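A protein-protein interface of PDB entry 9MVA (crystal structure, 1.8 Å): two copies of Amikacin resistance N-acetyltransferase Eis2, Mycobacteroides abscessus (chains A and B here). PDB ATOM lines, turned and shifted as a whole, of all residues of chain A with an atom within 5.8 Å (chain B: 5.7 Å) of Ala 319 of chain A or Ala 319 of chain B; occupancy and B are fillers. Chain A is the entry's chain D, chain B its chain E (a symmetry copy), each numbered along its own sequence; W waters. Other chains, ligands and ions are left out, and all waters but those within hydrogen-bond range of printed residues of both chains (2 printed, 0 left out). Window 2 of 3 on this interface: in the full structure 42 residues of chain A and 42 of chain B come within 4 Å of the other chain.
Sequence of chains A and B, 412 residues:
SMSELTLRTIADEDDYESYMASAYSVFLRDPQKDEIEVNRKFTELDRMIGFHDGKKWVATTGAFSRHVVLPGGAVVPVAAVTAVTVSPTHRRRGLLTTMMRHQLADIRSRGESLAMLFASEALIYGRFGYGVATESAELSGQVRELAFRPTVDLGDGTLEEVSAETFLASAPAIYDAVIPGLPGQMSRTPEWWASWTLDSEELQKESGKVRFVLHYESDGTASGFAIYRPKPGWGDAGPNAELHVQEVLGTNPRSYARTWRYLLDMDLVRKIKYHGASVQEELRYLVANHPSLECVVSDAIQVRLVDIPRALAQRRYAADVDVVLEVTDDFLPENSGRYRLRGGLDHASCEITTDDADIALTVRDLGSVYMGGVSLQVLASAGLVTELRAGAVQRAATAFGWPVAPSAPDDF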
ATOM      1  N   TYR A 317       8.336 -17.166  23.228  1.00  0.00           N
ATOM      2  CA  TYR A 317       9.284 -18.023  22.534  1.00  0.00           C
ATOM      3  C   TYR A 317       9.877 -17.277  21.351  1.00  0.00           C
ATOM      4  O   TYR A 317       9.203 -16.456  20.719  1.00  0.00           O
ATOM      5  CB  TYR A 317       8.595 -19.349  22.121  1.00  0.00           C
ATOM      6  CG  TYR A 317       8.225 -20.108  23.369  1.00  0.00           C
ATOM      7  CD1 TYR A 317       7.023 -19.858  24.035  1.00  0.00           C
ATOM      8  CD2 TYR A 317       9.116 -21.019  23.933  1.00  0.00           C
ATOM      9  CE1 TYR A 317       6.703 -20.530  25.215  1.00  0.00           C
ATOM     10  CE2 TYR A 317       8.803 -21.692  25.106  1.00  0.00           C
ATOM     11  CZ  TYR A 317       7.610 -21.439  25.745  1.00  0.00           C
ATOM     12  OH  TYR A 317       7.323 -22.116  26.920  1.00  0.00           O
ATOM     13  N   ALA A 318      11.164 -17.518  21.093  1.00  0.00           N
ATOM     14  CA  ALA A 318      11.876 -16.716  20.101  1.00  0.00           C
ATOM     15  C   ALA A 318      11.388 -16.991  18.691  1.00  0.00           C
ATOM     16  O   ALA A 318      11.663 -16.197  17.782  1.00  0.00           O
ATOM     17  CB  ALA A 318      13.386 -16.973  20.186  1.00  0.00           C
ATOM     18  N   ALA A 319      10.686 -18.102  18.490  1.00  0.00           N
ATOM     19  CA  ALA A 319      10.120 -18.439  17.192  1.00  0.00           C
ATOM     20  C   ALA A 319       8.971 -19.410  17.430  1.00  0.00           C
ATOM     21  O   ALA A 319       8.775 -19.906  18.543  1.00  0.00           O
ATOM     22  CB  ALA A 319      11.183 -19.025  16.259  1.00  0.00           C
ATOM     23  N   ASP A 320       8.200 -19.670  16.373  1.00  0.00           N
ATOM     24  CA  ASP A 320       7.051 -20.558  16.507  1.00  0.00           C
ATOM     25  C   ASP A 320       7.478 -21.969  16.892  1.00  0.00           C
ATOM     26  O   ASP A 320       8.496 -22.483  16.418  1.00  0.00           O
ATOM     27  CB  ASP A 320       6.255 -20.620  15.199  1.00  0.00           C
ATOM     28  CG  ASP A 320       5.616 -19.302  14.843  1.00  0.00           C
ATOM     29  OD1 ASP A 320       5.288 -18.527  15.767  1.00  0.00           O
ATOM     30  OD2 ASP A 320       5.434 -19.050  13.635  1.00  0.00           O
ATOM     31  N   VAL A 321       6.667 -22.602  17.734  1.00  0.00           N
ATOM     32  CA  VAL A 321       6.898 -23.976  18.161  1.00  0.00           C
ATOM     33  C   VAL A 321       5.550 -24.631  18.413  1.00  0.00           C
ATOM     34  O   VAL A 321       4.617 -23.999  18.915  1.00  0.00           O
ATOM     35  CB  VAL A 321       7.799 -24.042  19.417  1.00  0.00           C
ATOM     36  CG1 VAL A 321       7.144 -23.333  20.618  1.00  0.00           C
ATOM     37  CG2 VAL A 321       8.163 -25.486  19.748  1.00  0.00           C
ATOM     38  N   GLY A 343       3.627 -22.094  20.990  1.00  0.00           N
ATOM     39  CA  GLY A 343       4.144 -20.807  21.422  1.00  0.00           C
ATOM     40  C   GLY A 343       4.848 -20.072  20.306  1.00  0.00           C
ATOM     41  O   GLY A 343       5.082 -20.603  19.219  1.00  0.00           O
ATOM     42  N   GLY A 344       5.173 -18.822  20.605  1.00  0.00           N
ATOM     43  CA  GLY A 344       5.865 -17.979  19.656  1.00  0.00           C
ATOM     44  C   GLY A 344       6.095 -16.632  20.297  1.00  0.00           C
ATOM     45  O   GLY A 344       5.977 -16.493  21.513  1.00  0.00           O
ATOM     46  N   LEU A 345       6.400 -15.631  19.477  1.00  0.00           N
ATOM     47  CA  LEU A 345       6.684 -14.318  20.051  1.00  0.00           C
ATOM     48  C   LEU A 345       5.459 -13.706  20.713  1.00  0.00           C
ATOM     49  O   LEU A 345       5.594 -12.963  21.689  1.00  0.00           O
ATOM     50  CB  LEU A 345       7.221 -13.378  18.979  1.00  0.00           C
ATOM     51  CG  LEU A 345       8.682 -13.624  18.662  1.00  0.00           C
ATOM     52  CD1 LEU A 345       9.055 -12.880  17.389  1.00  0.00           C
ATOM     53  CD2 LEU A 345       9.538 -13.185  19.848  1.00  0.00           C
ATOM     54  N   THR A 398      15.376 -23.661  19.300  1.00  0.00           N
ATOM     55  CA  THR A 398      15.355 -22.263  18.890  1.00  0.00           C
ATOM     56  C   THR A 398      14.237 -21.496  19.590  1.00  0.00           C
ATOM     57  O   THR A 398      14.449 -20.373  20.062  1.00  0.00           O
ATOM     58  CB  THR A 398      15.228 -22.208  17.370  1.00  0.00           C
ATOM     59  OG1 THR A 398      16.448 -22.710  16.808  1.00  0.00           O
ATOM     60  CG2 THR A 398      14.965 -20.789  16.874  1.00  0.00           C
ATOM     61  N   ALA A 399      13.043 -22.089  19.681  1.00  0.00           N
ATOM     62  CA  ALA A 399      11.935 -21.414  20.353  1.00  0.00           C
ATOM     63  C   ALA A 399      12.242 -21.141  21.825  1.00  0.00           C
ATOM     64  O   ALA A 399      11.940 -20.055  22.335  1.00  0.00           O
ATOM     65  CB  ALA A 399      10.659 -22.247  20.222  1.00  0.00           C
ATOM     66  N   TYR B 317      19.116 -20.550   8.494  1.00  0.00           N
ATOM     67  CA  TYR B 317      18.701 -19.701   9.598  1.00  0.00           C
ATOM     68  C   TYR B 317      17.799 -20.471  10.550  1.00  0.00           C
ATOM     69  O   TYR B 317      17.008 -21.326  10.125  1.00  0.00           O
ATOM     70  CB  TYR B 317      18.022 -18.437   9.047  1.00  0.00           C
ATOM     71  CG  TYR B 317      19.042 -17.646   8.278  1.00  0.00           C
ATOM     72  CD1 TYR B 317      19.284 -17.908   6.939  1.00  0.00           C
ATOM     73  CD2 TYR B 317      19.837 -16.703   8.920  1.00  0.00           C
ATOM     74  CE1 TYR B 317      20.260 -17.227   6.243  1.00  0.00           C
ATOM     75  CE2 TYR B 317      20.812 -16.014   8.232  1.00  0.00           C
ATOM     76  CZ  TYR B 317      21.023 -16.274   6.905  1.00  0.00           C
ATOM     77  OH  TYR B 317      21.999 -15.577   6.228  1.00  0.00           O
ATOM     78  N   ALA B 318      17.953 -20.178  11.847  1.00  0.00           N
ATOM     79  CA  ALA B 318      17.311 -20.958  12.901  1.00  0.00           C
ATOM     80  C   ALA B 318      15.799 -20.822  12.870  1.00  0.00           C
ATOM     81  O   ALA B 318      15.096 -21.701  13.373  1.00  0.00           O
ATOM     82  CB  ALA B 318      17.838 -20.532  14.276  1.00  0.00           C
ATOM     83  N   ALA B 319      15.291 -19.738  12.302  1.00  0.00           N
ATOM     84  CA  ALA B 319      13.862 -19.538  12.120  1.00  0.00           C
ATOM     85  C   ALA B 319      13.707 -18.623  10.923  1.00  0.00           C
ATOM     86  O   ALA B 319      14.693 -18.098  10.402  1.00  0.00           O
ATOM     87  CB  ALA B 319      13.206 -18.941  13.364  1.00  0.00           C
ATOM     88  N   ASP B 320      12.460 -18.419  10.501  1.00  0.00           N
ATOM     89  CA  ASP B 320      12.201 -17.604   9.320  1.00  0.00           C
ATOM     90  C   ASP B 320      12.607 -16.154   9.536  1.00  0.00           C
ATOM     91  O   ASP B 320      12.426 -15.586  10.617  1.00  0.00           O
ATOM     92  CB  ASP B 320      10.722 -17.645   8.948  1.00  0.00           C
ATOM     93  CG  ASP B 320      10.274 -19.010   8.502  1.00  0.00           C
ATOM     94  OD1 ASP B 320      11.103 -19.759   7.935  1.00  0.00           O
ATOM     95  OD2 ASP B 320       9.087 -19.326   8.718  1.00  0.00           O
ATOM     96  N   VAL B 321      13.109 -15.530   8.482  1.00  0.00           N
ATOM     97  CA  VAL B 321      13.456 -14.117   8.554  1.00  0.00           C
ATOM     98  C   VAL B 321      13.234 -13.483   7.188  1.00  0.00           C
ATOM     99  O   VAL B 321      13.460 -14.106   6.146  1.00  0.00           O
ATOM    100  CB  VAL B 321      14.909 -13.927   9.041  1.00  0.00           C
ATOM    101  CG1 VAL B 321      15.896 -14.558   8.059  1.00  0.00           C
ATOM    102  CG2 VAL B 321      15.222 -12.448   9.253  1.00  0.00           C
ATOM    103  N   GLY B 343      15.214 -16.013   4.658  1.00  0.00           N
ATOM    104  CA  GLY B 343      15.834 -17.265   5.040  1.00  0.00           C
ATOM    105  C   GLY B 343      15.011 -18.015   6.059  1.00  0.00           C
ATOM    106  O   GLY B 343      14.017 -17.520   6.596  1.00  0.00           O
ATOM    107  N   GLY B 344      15.461 -19.232   6.317  1.00  0.00           N
ATOM    108  CA  GLY B 344      14.838 -20.070   7.316  1.00  0.00           C
ATOM    109  C   GLY B 344      15.614 -21.359   7.377  1.00  0.00           C
ATOM    110  O   GLY B 344      16.743 -21.431   6.892  1.00  0.00           O
ATOM    111  N   LEU B 345      14.998 -22.395   7.955  1.00  0.00           N
ATOM    112  CA  LEU B 345      15.728 -23.648   8.088  1.00  0.00           C
ATOM    113  C   LEU B 345      16.007 -24.281   6.739  1.00  0.00           C
ATOM    114  O   LEU B 345      16.994 -25.007   6.588  1.00  0.00           O
ATOM    115  CB  LEU B 345      14.955 -24.617   8.971  1.00  0.00           C
ATOM    116  CG  LEU B 345      15.068 -24.307  10.464  1.00  0.00           C
ATOM    117  CD1 LEU B 345      14.028 -25.101  11.247  1.00  0.00           C
ATOM    118  CD2 LEU B 345      16.478 -24.641  10.959  1.00  0.00           C
ATOM    119  N   THR B 398      17.216 -13.941  16.229  1.00  0.00           N
ATOM    120  CA  THR B 398      16.918 -15.362  16.354  1.00  0.00           C
ATOM    121  C   THR B 398      17.335 -16.121  15.098  1.00  0.00           C
ATOM    122  O   THR B 398      17.941 -17.192  15.187  1.00  0.00           O
ATOM    123  CB  THR B 398      15.432 -15.533  16.657  1.00  0.00           C
ATOM    124  OG1 THR B 398      15.147 -14.913  17.919  1.00  0.00           O
ATOM    125  CG2 THR B 398      15.025 -17.021  16.680  1.00  0.00           C
ATOM    126  N   ALA B 399      17.065 -15.557  13.915  1.00  0.00           N
ATOM    127  CA  ALA B 399      17.397 -16.255  12.676  1.00  0.00           C
ATOM    128  C   ALA B 399      18.903 -16.438  12.511  1.00  0.00           C
ATOM    129  O   ALA B 399      19.364 -17.514  12.108  1.00  0.00           O
ATOM    130  CB  ALA B 399      16.823 -15.502  11.478  1.00  0.00           C
HETATM  131  O   HOH W   1      12.721 -13.718  18.229  1.00  0.00           O
HETATM  132  O   HOH W   2      16.132 -23.958  14.470  1.00  0.00           O
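N of Ala 318 of chain A is in hydrogen-bond range of O of Ala 399 of chain A (2.9 Å).
The backbone NH of Ala 318 of chain B is in hydrogen-bond range of the backbone carbonyl oxygen of Ala 399 of chain B (3.0 Å).
Thr 398 of chain B touches Ala 318 of chain A.
Ala 319 of chain A touches Ala 319 of chain B (CB to CB, 3.5 Å).
CB of Ala 318 of chain B touches OG1 of Thr 398 of chain A, 3.6 Å away.
Thr 398 of chain A touches Thr 398 of chain B.
Of the printed residues of chain B, Ala 318 of chain A touches Thr 398.
Printed residues of chain B within 4 Å of Ala 319 of chain A: Ala 319 (3.5 Å).
Asp 320 of chain A touches none of the printed residues of chain B.
Of the printed residues of chain A, Ala 318 of chain B touches Thr 398 (3.6 Å).
Of chain A, only Ala 319 (3.5 Å) comes within 4 Å of Ala 319 of chain B.
Printed residues of chain A within 4 Å of Thr 398 of chain B: Ala 318 (3.5 Å) and Thr 398 (3.8 Å).
Ala 399 of chain B touches none of the printed residues of chain A.
Among the printed residues, 4 pairs touch across the chains.
Among the printed residues, no Asp or Glu carboxylate lies within 4 Å of a Lys or Arg side-chain nitrogen of the other chain.
Ala 318 of chain A touches Thr 398 of chain B, and with the chains exchanged Thr 398 of chain A touches Ala 318 of chain B.
Ala 319 of chain B touches its own counterpart, Ala 319 of chain A.
Thr 398 of chain A touches its own counterpart, Thr 398 of chain B.
10 positions are printed for both chains.
Water W2 bridges OG1 of Thr 398 of chain A (2.7 Å) and O of Ala 318 of chain B (2.7 Å).
Water W1 bridges the side-chain hydroxyl of Thr 398 of chain B (2.7 Å) and the backbone carbonyl oxygen of Ala 318 of chain A (2.7 Å).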
